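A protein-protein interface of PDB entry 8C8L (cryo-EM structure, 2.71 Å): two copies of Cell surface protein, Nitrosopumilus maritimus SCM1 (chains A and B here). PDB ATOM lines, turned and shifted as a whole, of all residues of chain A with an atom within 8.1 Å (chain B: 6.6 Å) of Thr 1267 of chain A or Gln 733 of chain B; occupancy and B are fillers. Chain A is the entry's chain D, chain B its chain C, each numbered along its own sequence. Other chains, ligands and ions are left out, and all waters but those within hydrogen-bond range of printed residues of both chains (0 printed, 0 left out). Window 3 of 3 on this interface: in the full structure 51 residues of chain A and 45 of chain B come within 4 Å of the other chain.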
ATOM      1  N   LEU A1064     -15.057  10.888 -13.382  1.00  0.00           N
ATOM      2  CA  LEU A1064     -15.151  11.681 -12.137  1.00  0.00           C
ATOM      3  C   LEU A1064     -13.799  12.339 -11.906  1.00  0.00           C
ATOM      4  O   LEU A1064     -12.764  11.772 -12.253  1.00  0.00           O
ATOM      5  CB  LEU A1064     -15.562  10.783 -10.968  1.00  0.00           C
ATOM      6  CG  LEU A1064     -16.984  10.209 -11.025  1.00  0.00           C
ATOM      7  CD1 LEU A1064     -17.230   9.336  -9.818  1.00  0.00           C
ATOM      8  CD2 LEU A1064     -18.065  11.282 -11.146  1.00  0.00           C
ATOM      9  N   PRO A1065     -13.766  13.587 -11.393  1.00  0.00           N
ATOM     10  CA  PRO A1065     -12.498  14.224 -11.042  1.00  0.00           C
ATOM     11  C   PRO A1065     -11.685  13.376 -10.047  1.00  0.00           C
ATOM     12  O   PRO A1065     -12.216  12.450  -9.451  1.00  0.00           O
ATOM     13  CB  PRO A1065     -12.881  15.594 -10.457  1.00  0.00           C
ATOM     14  CG  PRO A1065     -14.409  15.633 -10.396  1.00  0.00           C
ATOM     15  CD  PRO A1065     -14.933  14.458 -11.195  1.00  0.00           C
ATOM     16  N   THR A1066     -10.400  13.693  -9.919  1.00  0.00           N
ATOM     17  CA  THR A1066      -9.432  12.913  -9.103  1.00  0.00           C
ATOM     18  C   THR A1066     -10.002  12.719  -7.693  1.00  0.00           C
ATOM     19  O   THR A1066     -10.433  13.714  -7.077  1.00  0.00           O
ATOM     20  CB  THR A1066      -8.036  13.547  -9.062  1.00  0.00           C
ATOM     21  OG1 THR A1066      -7.243  12.654  -8.280  1.00  0.00           O
ATOM     22  CG2 THR A1066      -7.980  14.939  -8.469  1.00  0.00           C
ATOM     23  N   PHE A1258     -17.545   6.570  -1.895  1.00  0.00           N
ATOM     24  CA  PHE A1258     -17.558   7.985  -2.327  1.00  0.00           C
ATOM     25  C   PHE A1258     -17.412   8.954  -1.162  1.00  0.00           C
ATOM     26  O   PHE A1258     -17.096  10.124  -1.438  1.00  0.00           O
ATOM     27  CB  PHE A1258     -18.843   8.253  -3.098  1.00  0.00           C
ATOM     28  CG  PHE A1258     -18.847   7.720  -4.503  1.00  0.00           C
ATOM     29  CD1 PHE A1258     -17.676   7.341  -5.149  1.00  0.00           C
ATOM     30  CD2 PHE A1258     -20.046   7.593  -5.186  1.00  0.00           C
ATOM     31  CE1 PHE A1258     -17.710   6.865  -6.452  1.00  0.00           C
ATOM     32  CE2 PHE A1258     -20.076   7.109  -6.485  1.00  0.00           C
ATOM     33  CZ  PHE A1258     -18.907   6.756  -7.118  1.00  0.00           C
ATOM     34  N   SER A1264     -16.906  17.151   4.834  1.00  0.00           N
ATOM     35  CA  SER A1264     -17.673  17.800   3.743  1.00  0.00           C
ATOM     36  C   SER A1264     -18.662  16.821   3.114  1.00  0.00           C
ATOM     37  O   SER A1264     -18.472  15.586   3.231  1.00  0.00           O
ATOM     38  CB  SER A1264     -16.754  18.398   2.711  1.00  0.00           C
ATOM     39  OG  SER A1264     -16.488  17.479   1.666  1.00  0.00           O
ATOM     40  N   ALA A1265     -19.667  17.382   2.445  1.00  0.00           N
ATOM     41  CA  ALA A1265     -20.614  16.653   1.576  1.00  0.00           C
ATOM     42  C   ALA A1265     -20.063  16.602   0.151  1.00  0.00           C
ATOM     43  O   ALA A1265     -19.905  17.676  -0.463  1.00  0.00           O
ATOM     44  CB  ALA A1265     -21.965  17.313   1.628  1.00  0.00           C
ATOM     45  N   GLU A1266     -19.777  15.404  -0.348  1.00  0.00           N
ATOM     46  CA  GLU A1266     -19.095  15.215  -1.654  1.00  0.00           C
ATOM     47  C   GLU A1266     -20.143  15.272  -2.770  1.00  0.00           C
ATOM     48  O   GLU A1266     -21.270  14.797  -2.604  1.00  0.00           O
ATOM     49  CB  GLU A1266     -18.263  13.927  -1.710  1.00  0.00           C
ATOM     50  CG  GLU A1266     -17.133  13.854  -0.669  1.00  0.00           C
ATOM     51  CD  GLU A1266     -17.606  13.427   0.713  1.00  0.00           C
ATOM     52  OE1 GLU A1266     -18.820  13.163   0.799  1.00  0.00           O
ATOM     53  OE2 GLU A1266     -16.808  13.376   1.672  1.00  0.00           O
ATOM     54  N   THR A1267     -19.763  15.843  -3.894  1.00  0.00           N
ATOM     55  CA  THR A1267     -20.643  15.983  -5.075  1.00  0.00           C
ATOM     56  C   THR A1267     -20.113  15.107  -6.210  1.00  0.00           C
ATOM     57  O   THR A1267     -18.890  15.144  -6.488  1.00  0.00           O
ATOM     58  CB  THR A1267     -20.734  17.452  -5.494  1.00  0.00           C
ATOM     59  OG1 THR A1267     -20.837  18.263  -4.322  1.00  0.00           O
ATOM     60  CG2 THR A1267     -21.905  17.691  -6.415  1.00  0.00           C
ATOM     61  N   TYR A1268     -21.001  14.384  -6.880  1.00  0.00           N
ATOM     62  CA  TYR A1268     -20.610  13.458  -7.972  1.00  0.00           C
ATOM     63  C   TYR A1268     -21.484  13.705  -9.188  1.00  0.00           C
ATOM     64  O   TYR A1268     -22.669  14.026  -9.035  1.00  0.00           O
ATOM     65  CB  TYR A1268     -20.647  12.005  -7.500  1.00  0.00           C
ATOM     66  CG  TYR A1268     -19.524  11.708  -6.546  1.00  0.00           C
ATOM     67  CD1 TYR A1268     -18.213  11.624  -6.990  1.00  0.00           C
ATOM     68  CD2 TYR A1268     -19.754  11.601  -5.185  1.00  0.00           C
ATOM     69  CE1 TYR A1268     -17.164  11.393  -6.112  1.00  0.00           C
ATOM     70  CE2 TYR A1268     -18.715  11.398  -4.294  1.00  0.00           C
ATOM     71  CZ  TYR A1268     -17.416  11.287  -4.753  1.00  0.00           C
ATOM     72  OH  TYR A1268     -16.419  11.055  -3.847  1.00  0.00           O
ATOM     73  N   ASP A1269     -20.879  13.549 -10.361  1.00  0.00           N
ATOM     74  CA  ASP A1269     -21.515  13.812 -11.675  1.00  0.00           C
ATOM     75  C   ASP A1269     -22.740  12.907 -11.809  1.00  0.00           C
ATOM     76  O   ASP A1269     -22.695  11.775 -11.334  1.00  0.00           O
ATOM     77  CB  ASP A1269     -20.534  13.586 -12.828  1.00  0.00           C
ATOM     78  CG  ASP A1269     -21.118  13.923 -14.183  1.00  0.00           C
ATOM     79  OD1 ASP A1269     -22.346  13.713 -14.371  1.00  0.00           O
ATOM     80  OD2 ASP A1269     -20.341  14.386 -15.048  1.00  0.00           O
ATOM     81  N   LEU A1270     -23.783  13.398 -12.464  1.00  0.00           N
ATOM     82  CA  LEU A1270     -25.049  12.647 -12.658  1.00  0.00           C
ATOM     83  C   LEU A1270     -24.944  11.751 -13.896  1.00  0.00           C
ATOM     84  O   LEU A1270     -25.828  10.904 -14.043  1.00  0.00           O
ATOM     85  CB  LEU A1270     -26.208  13.647 -12.760  1.00  0.00           C
ATOM     86  CG  LEU A1270     -27.626  13.095 -12.956  1.00  0.00           C
ATOM     87  CD1 LEU A1270     -28.118  12.265 -11.773  1.00  0.00           C
ATOM     88  CD2 LEU A1270     -28.579  14.241 -13.202  1.00  0.00           C
ATOM     89  N   LEU A1272     -23.139   9.233 -14.321  1.00  0.00           N
ATOM     90  CA  LEU A1272     -22.933   7.829 -13.856  1.00  0.00           C
ATOM     91  C   LEU A1272     -24.179   6.967 -14.068  1.00  0.00           C
ATOM     92  O   LEU A1272     -24.007   5.759 -14.290  1.00  0.00           O
ATOM     93  CB  LEU A1272     -22.574   7.803 -12.369  1.00  0.00           C
ATOM     94  CG  LEU A1272     -21.205   8.381 -12.013  1.00  0.00           C
ATOM     95  CD1 LEU A1272     -20.995   8.427 -10.504  1.00  0.00           C
ATOM     96  CD2 LEU A1272     -20.082   7.608 -12.697  1.00  0.00           C
ATOM     97  N   PRO A1300     -30.552  18.784  -6.764  1.00  0.00           N
ATOM     98  CA  PRO A1300     -29.627  19.730  -7.390  1.00  0.00           C
ATOM     99  C   PRO A1300     -29.118  19.258  -8.760  1.00  0.00           C
ATOM    100  O   PRO A1300     -29.678  18.367  -9.329  1.00  0.00           O
ATOM    101  CB  PRO A1300     -28.491  19.887  -6.361  1.00  0.00           C
ATOM    102  CG  PRO A1300     -28.596  18.702  -5.434  1.00  0.00           C
ATOM    103  CD  PRO A1300     -29.975  18.117  -5.592  1.00  0.00           C
ATOM    104  N   THR A1301     -28.058  19.862  -9.275  1.00  0.00           N
ATOM    105  CA  THR A1301     -27.571  19.562 -10.641  1.00  0.00           C
ATOM    106  C   THR A1301     -27.054  18.132 -10.711  1.00  0.00           C
ATOM    107  O   THR A1301     -26.973  17.609 -11.829  1.00  0.00           O
ATOM    108  CB  THR A1301     -26.500  20.563 -11.061  1.00  0.00           C
ATOM    109  OG1 THR A1301     -25.374  20.413 -10.195  1.00  0.00           O
ATOM    110  CG2 THR A1301     -27.047  21.968 -10.995  1.00  0.00           C
ATOM    111  N   ASP A1302     -26.712  17.532  -9.572  1.00  0.00           N
ATOM    112  CA  ASP A1302     -26.138  16.166  -9.541  1.00  0.00           C
ATOM    113  C   ASP A1302     -26.199  15.597  -8.122  1.00  0.00           C
ATOM    114  O   ASP A1302     -26.757  16.249  -7.230  1.00  0.00           O
ATOM    115  CB  ASP A1302     -24.716  16.206 -10.096  1.00  0.00           C
ATOM    116  CG  ASP A1302     -23.783  17.066  -9.268  1.00  0.00           C
ATOM    117  OD1 ASP A1302     -24.268  17.712  -8.318  1.00  0.00           O
ATOM    118  OD2 ASP A1302     -22.571  17.073  -9.571  1.00  0.00           O
ATOM    119  N   PHE A1303     -25.620  14.422  -7.918  1.00  0.00           N
ATOM    120  CA  PHE A1303     -25.719  13.699  -6.629  1.00  0.00           C
ATOM    121  C   PHE A1303     -25.071  14.508  -5.507  1.00  0.00           C
ATOM    122  O   PHE A1303     -24.127  15.253  -5.766  1.00  0.00           O
ATOM    123  CB  PHE A1303     -25.078  12.320  -6.735  1.00  0.00           C
ATOM    124  CG  PHE A1303     -25.999  11.295  -7.331  1.00  0.00           C
ATOM    125  CD1 PHE A1303     -25.921  10.976  -8.675  1.00  0.00           C
ATOM    126  CD2 PHE A1303     -26.972  10.684  -6.556  1.00  0.00           C
ATOM    127  CE1 PHE A1303     -26.789  10.048  -9.227  1.00  0.00           C
ATOM    128  CE2 PHE A1303     -27.823   9.740  -7.104  1.00  0.00           C
ATOM    129  CZ  PHE A1303     -27.741   9.436  -8.443  1.00  0.00           C
ATOM    130  N   ARG A1304     -25.573  14.349  -4.292  1.00  0.00           N
ATOM    131  CA  ARG A1304     -25.074  15.072  -3.101  1.00  0.00           C
ATOM    132  C   ARG A1304     -25.335  14.248  -1.848  1.00  0.00           C
ATOM    133  O   ARG A1304     -26.396  13.633  -1.783  1.00  0.00           O
ATOM    134  CB  ARG A1304     -25.793  16.413  -2.987  1.00  0.00           C
ATOM    135  CG  ARG A1304     -25.221  17.311  -1.893  1.00  0.00           C
ATOM    136  CD  ARG A1304     -25.792  18.721  -1.909  1.00  0.00           C
ATOM    137  NE  ARG A1304     -25.507  19.388  -3.174  1.00  0.00           N
ATOM    138  CZ  ARG A1304     -24.309  19.804  -3.561  1.00  0.00           C
ATOM    139  NH1 ARG A1304     -23.268  19.660  -2.766  1.00  0.00           N
ATOM    140  NH2 ARG A1304     -24.149  20.365  -4.741  1.00  0.00           N
ATOM    141  N   GLU A1305     -24.418  14.262  -0.886  1.00  0.00           N
ATOM    142  CA  GLU A1305     -24.567  13.488   0.368  1.00  0.00           C
ATOM    143  C   GLU A1305     -25.723  14.063   1.199  1.00  0.00           C
ATOM    144  O   GLU A1305     -25.963  15.281   1.141  1.00  0.00           O
ATOM    145  CB  GLU A1305     -23.312  13.570   1.225  1.00  0.00           C
ATOM    146  CG  GLU A1305     -22.364  12.388   1.184  1.00  0.00           C
ATOM    147  CD  GLU A1305     -21.245  12.579   2.188  1.00  0.00           C
ATOM    148  OE1 GLU A1305     -20.741  11.623   2.817  1.00  0.00           O
ATOM    149  OE2 GLU A1305     -20.894  13.725   2.372  1.00  0.00           O
ATOM    150  N   PHE A1313     -26.344   9.322  -1.179  1.00  0.00           N
ATOM    151  CA  PHE A1313     -26.513  10.449  -2.125  1.00  0.00           C
ATOM    152  C   PHE A1313     -27.933  10.443  -2.680  1.00  0.00           C
ATOM    153  O   PHE A1313     -28.455   9.368  -3.012  1.00  0.00           O
ATOM    154  CB  PHE A1313     -25.490  10.365  -3.254  1.00  0.00           C
ATOM    155  CG  PHE A1313     -24.064  10.371  -2.780  1.00  0.00           C
ATOM    156  CD1 PHE A1313     -23.480   9.213  -2.286  1.00  0.00           C
ATOM    157  CD2 PHE A1313     -23.294  11.527  -2.836  1.00  0.00           C
ATOM    158  CE1 PHE A1313     -22.170   9.212  -1.832  1.00  0.00           C
ATOM    159  CE2 PHE A1313     -21.978  11.520  -2.396  1.00  0.00           C
ATOM    160  CZ  PHE A1313     -21.420  10.363  -1.893  1.00  0.00           C
ATOM    161  N   THR B 728     -10.557  27.647  -7.232  1.00  0.00           N
ATOM    162  CA  THR B 728      -9.894  26.993  -8.393  1.00  0.00           C
ATOM    163  C   THR B 728     -10.853  25.968  -9.002  1.00  0.00           C
ATOM    164  O   THR B 728     -11.612  25.360  -8.234  1.00  0.00           O
ATOM    165  CB  THR B 728      -8.585  26.322  -7.974  1.00  0.00           C
ATOM    166  OG1 THR B 728      -8.879  25.286  -7.040  1.00  0.00           O
ATOM    167  CG2 THR B 728      -7.606  27.284  -7.348  1.00  0.00           C
ATOM    168  N   ASP B 729     -10.808  25.783 -10.323  1.00  0.00           N
ATOM    169  CA  ASP B 729     -11.688  24.836 -11.059  1.00  0.00           C
ATOM    170  C   ASP B 729     -13.162  25.235 -10.850  1.00  0.00           C
ATOM    171  O   ASP B 729     -13.497  26.422 -10.972  1.00  0.00           O
ATOM    172  CB  ASP B 729     -11.342  23.421 -10.593  1.00  0.00           C
ATOM    173  CG  ASP B 729     -11.778  22.296 -11.520  1.00  0.00           C
ATOM    174  OD1 ASP B 729     -12.643  21.530 -11.078  1.00  0.00           O
ATOM    175  OD2 ASP B 729     -11.243  22.209 -12.654  1.00  0.00           O
ATOM    176  N   ASP B 730     -14.026  24.262 -10.553  1.00  0.00           N
ATOM    177  CA  ASP B 730     -15.466  24.455 -10.249  1.00  0.00           C
ATOM    178  C   ASP B 730     -15.602  25.268  -8.942  1.00  0.00           C
ATOM    179  O   ASP B 730     -16.496  26.108  -8.862  1.00  0.00           O
ATOM    180  CB  ASP B 730     -16.184  23.092 -10.252  1.00  0.00           C
ATOM    181  CG  ASP B 730     -15.403  21.979  -9.553  1.00  0.00           C
ATOM    182  OD1 ASP B 730     -14.711  22.321  -8.629  1.00  0.00           O
ATOM    183  OD2 ASP B 730     -15.413  20.790  -9.951  1.00  0.00           O
ATOM    184  N   GLY B 731     -14.735  25.028  -7.958  1.00  0.00           N
ATOM    185  CA  GLY B 731     -14.841  25.574  -6.594  1.00  0.00           C
ATOM    186  C   GLY B 731     -15.854  24.791  -5.783  1.00  0.00           C
ATOM    187  O   GLY B 731     -16.247  25.260  -4.725  1.00  0.00           O
ATOM    188  N   VAL B 732     -16.263  23.624  -6.269  1.00  0.00           N
ATOM    189  CA  VAL B 732     -17.306  22.782  -5.619  1.00  0.00           C
ATOM    190  C   VAL B 732     -16.700  22.076  -4.403  1.00  0.00           C
ATOM    191  O   VAL B 732     -17.355  22.066  -3.350  1.00  0.00           O
ATOM    192  CB  VAL B 732     -17.926  21.790  -6.615  1.00  0.00           C
ATOM    193  CG1 VAL B 732     -18.827  20.771  -5.930  1.00  0.00           C
ATOM    194  CG2 VAL B 732     -18.695  22.533  -7.700  1.00  0.00           C
ATOM    195  N   GLN B 733     -15.500  21.509  -4.528  1.00  0.00           N
ATOM    196  CA  GLN B 733     -14.842  20.793  -3.399  1.00  0.00           C
ATOM    197  C   GLN B 733     -14.241  21.828  -2.438  1.00  0.00           C
ATOM    198  O   GLN B 733     -13.781  22.888  -2.895  1.00  0.00           O
ATOM    199  CB  GLN B 733     -13.776  19.823  -3.905  1.00  0.00           C
ATOM    200  CG  GLN B 733     -14.330  18.520  -4.473  1.00  0.00           C
ATOM    201  CD  GLN B 733     -15.095  18.658  -5.771  1.00  0.00           C
ATOM    202  OE1 GLN B 733     -14.628  19.254  -6.746  1.00  0.00           O
ATOM    203  NE2 GLN B 733     -16.269  18.052  -5.813  1.00  0.00           N
ATOM    204  N   SER B 734     -14.246  21.537  -1.137  1.00  0.00           N
ATOM    205  CA  SER B 734     -13.786  22.465  -0.068  1.00  0.00           C
ATOM    206  C   SER B 734     -12.294  22.778  -0.236  1.00  0.00           C
ATOM    207  O   SER B 734     -11.899  23.962  -0.120  1.00  0.00           O
ATOM    208  CB  SER B 734     -14.097  21.904   1.295  1.00  0.00           C
ATOM    209  OG  SER B 734     -15.512  21.825   1.498  1.00  0.00           O
ATOM    210  N   SER B 735     -11.498  21.764  -0.558  1.00  0.00           N
ATOM    211  CA  SER B 735     -10.041  21.904  -0.793  1.00  0.00           C
ATOM    212  C   SER B 735      -9.798  22.892  -1.934  1.00  0.00           C
ATOM    213  O   SER B 735      -8.645  23.275  -2.145  1.00  0.00           O
ATOM    214  CB  SER B 735      -9.429  20.576  -1.096  1.00  0.00           C
ATOM    215  OG  SER B 735     -10.162  19.930  -2.121  1.00  0.00           O
ATOM    216  N   GLU B 736     -10.841  23.267  -2.667  1.00  0.00           N
ATOM    217  CA  GLU B 736     -10.661  24.080  -3.886  1.00  0.00           C
ATOM    218  C   GLU B 736     -11.016  25.539  -3.615  1.00  0.00           C
ATOM    219  O   GLU B 736     -10.839  26.334  -4.528  1.00  0.00           O
ATOM    220  CB  GLU B 736     -11.430  23.469  -5.052  1.00  0.00           C
ATOM    221  CG  GLU B 736     -10.731  22.253  -5.621  1.00  0.00           C
ATOM    222  CD  GLU B 736     -11.465  21.535  -6.741  1.00  0.00           C
ATOM    223  OE1 GLU B 736     -11.235  21.816  -7.904  1.00  0.00           O
ATOM    224  OE2 GLU B 736     -12.278  20.665  -6.465  1.00  0.00           O
ATOM    225  N   ARG B 737     -11.426  25.879  -2.396  1.00  0.00           N
ATOM    226  CA  ARG B 737     -11.770  27.270  -2.004  1.00  0.00           C
ATOM    227  C   ARG B 737     -10.733  27.808  -1.025  1.00  0.00           C
ATOM    228  O   ARG B 737     -10.393  27.065  -0.087  1.00  0.00           O
ATOM    229  CB  ARG B 737     -13.140  27.264  -1.343  1.00  0.00           C
ATOM    230  CG  ARG B 737     -14.194  26.550  -2.170  1.00  0.00           C
ATOM    231  CD  ARG B 737     -15.596  26.935  -1.767  1.00  0.00           C
ATOM    232  NE  ARG B 737     -16.193  25.920  -0.919  1.00  0.00           N
ATOM    233  CZ  ARG B 737     -17.207  25.115  -1.240  1.00  0.00           C
ATOM    234  NH1 ARG B 737     -17.779  25.156  -2.434  1.00  0.00           N
ATOM    235  NH2 ARG B 737     -17.645  24.251  -0.341  1.00  0.00           N
ATOM    236  N   GLU B 793     -16.565  29.949   3.053  1.00  0.00           N
ATOM    237  CA  GLU B 793     -17.532  28.841   3.282  1.00  0.00           C
ATOM    238  C   GLU B 793     -17.900  28.768   4.763  1.00  0.00           C
ATOM    239  O   GLU B 793     -17.274  29.491   5.551  1.00  0.00           O
ATOM    240  CB  GLU B 793     -16.925  27.527   2.816  1.00  0.00           C
ATOM    241  CG  GLU B 793     -15.642  27.136   3.532  1.00  0.00           C
ATOM    242  CD  GLU B 793     -15.100  25.775   3.153  1.00  0.00           C
ATOM    243  OE1 GLU B 793     -15.904  24.883   2.820  1.00  0.00           O
ATOM    244  OE2 GLU B 793     -13.865  25.600   3.204  1.00  0.00           O
ATOM    245  N   SER B 885     -19.551  23.361 -13.509  1.00  0.00           N
ATOM    246  CA  SER B 885     -20.246  22.052 -13.401  1.00  0.00           C
ATOM    247  C   SER B 885     -21.696  22.249 -12.946  1.00  0.00           C
ATOM    248  O   SER B 885     -22.600  21.671 -13.564  1.00  0.00           O
ATOM    249  CB  SER B 885     -19.506  21.123 -12.478  1.00  0.00           C
ATOM    250  OG  SER B 885     -20.189  19.883 -12.360  1.00  0.00           O
ATOM    251  N   GLU B 999     -22.632  24.326   0.236  1.00  0.00           N
ATOM    252  CA  GLU B 999     -22.646  23.676  -1.079  1.00  0.00           C
ATOM    253  C   GLU B 999     -23.712  24.340  -1.965  1.00  0.00           C
ATOM    254  O   GLU B 999     -24.543  25.034  -1.425  1.00  0.00           O
ATOM    255  CB  GLU B 999     -22.829  22.188  -0.797  1.00  0.00           C
ATOM    256  CG  GLU B 999     -21.525  21.421  -0.975  1.00  0.00           C
ATOM    257  CD  GLU B 999     -20.505  21.377   0.129  1.00  0.00           C
ATOM    258  OE1 GLU B 999     -20.858  20.856   1.170  1.00  0.00           O
ATOM    259  OE2 GLU B 999     -19.357  21.805  -0.102  1.00  0.00           O
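Among the printed residues, merely in contact across the chains: Arg 1304 of chain A with Glu 999 of chain B (3.1 Å), Thr 1267 of chain A with Val 732 of chain B (3.6 Å), Ala 1265 of chain A with Glu 999 of chain B (3.7 Å), Ser 1264 of chain A with Ser 734 of chain B (3.8 Å) and Thr 1267 of chain A with Gln 733 of chain B (3.97 Å).
No position is printed for both chains.
Of the 5 pairs that touch across the chains among the printed residues, none has its exchanged pair printed and touching as well.
Of the printed residues of chain B, Ser 1264 of chain A touches Ser 734.
Printed residues of chain B within 4 Å of Ala 1265 of chain A: Glu 999 (3.7 Å).
Thr 1267 of chain A touches just these residues of chain B: Val 732 and Gln 733.
Printed residues of chain B within 4 Å of Arg 1304 of chain A: Glu 999 (3.1 Å).
Gln 733 of chain B touches just one residue of chain A: Thr 1267 (3.97 Å).
Printed residues of chain A within 4 Å of Ser 734 of chain B: Ser 1264 (3.8 Å).
Of the printed residues of chain A, Glu 999 of chain B touches Ala 1265 and Arg 1304.
The nearest residue of chain B that does not touch Thr 1267 of chain A is Glu 999 of chain B (4.7 Å).
The nearest residue of chain A that does not touch Gln 733 of chain B is Pro 1065 of chain A (5.1 Å).
Hydrophobic or aromatic side chains of chain B within 4 Å of the printed part of chain A: Val 732.
Along chain B the printed residues that touch a printed residue of chain A span positions 732 to 999.
Printed residues of chain A that touch a printed residue of chain B: Ser 1264, Ala 1265, Thr 1267 and Arg 1304.
Hydrophobic or aromatic side chains of chain A within 4 Å of the printed part of chain B: Ala 1265.
Among the printed residues, no Asp or Glu carboxylate lies within 4 Å of a Lys or Arg side-chain nitrogen of the other chain.
The side-chain amide oxygen of Gln 733 of chain B sits close to the side-chain carboxylate of Glu 736 of chain B.
The side-chain carboxylate (OD1) of Asp 730 of chain B lies within hydrogen-bond range of the backbone NH (N) of Val 732 of chain B (3.1 Å).
The guanidinium group (NH1) of Arg 1304 of chain A sits at hydrogen-bond distance from the side-chain hydroxyl (OG1) of Thr 1267 of chain A (3.2 Å).
The guanidinium group (NH2) of Arg 737 of chain B is in salt-bridge range of the side-chain carboxylate (OE2) of Glu 999 of chain B (3.0 Å).
NH1 of Arg 737 of chain B sits at hydrogen-bond distance from O of Val 732 of chain B, at 3.3 Å.
OG of Ser 734 of chain B sits at hydrogen-bond distance from OE1 of Glu 793 of chain B (3.4 Å).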
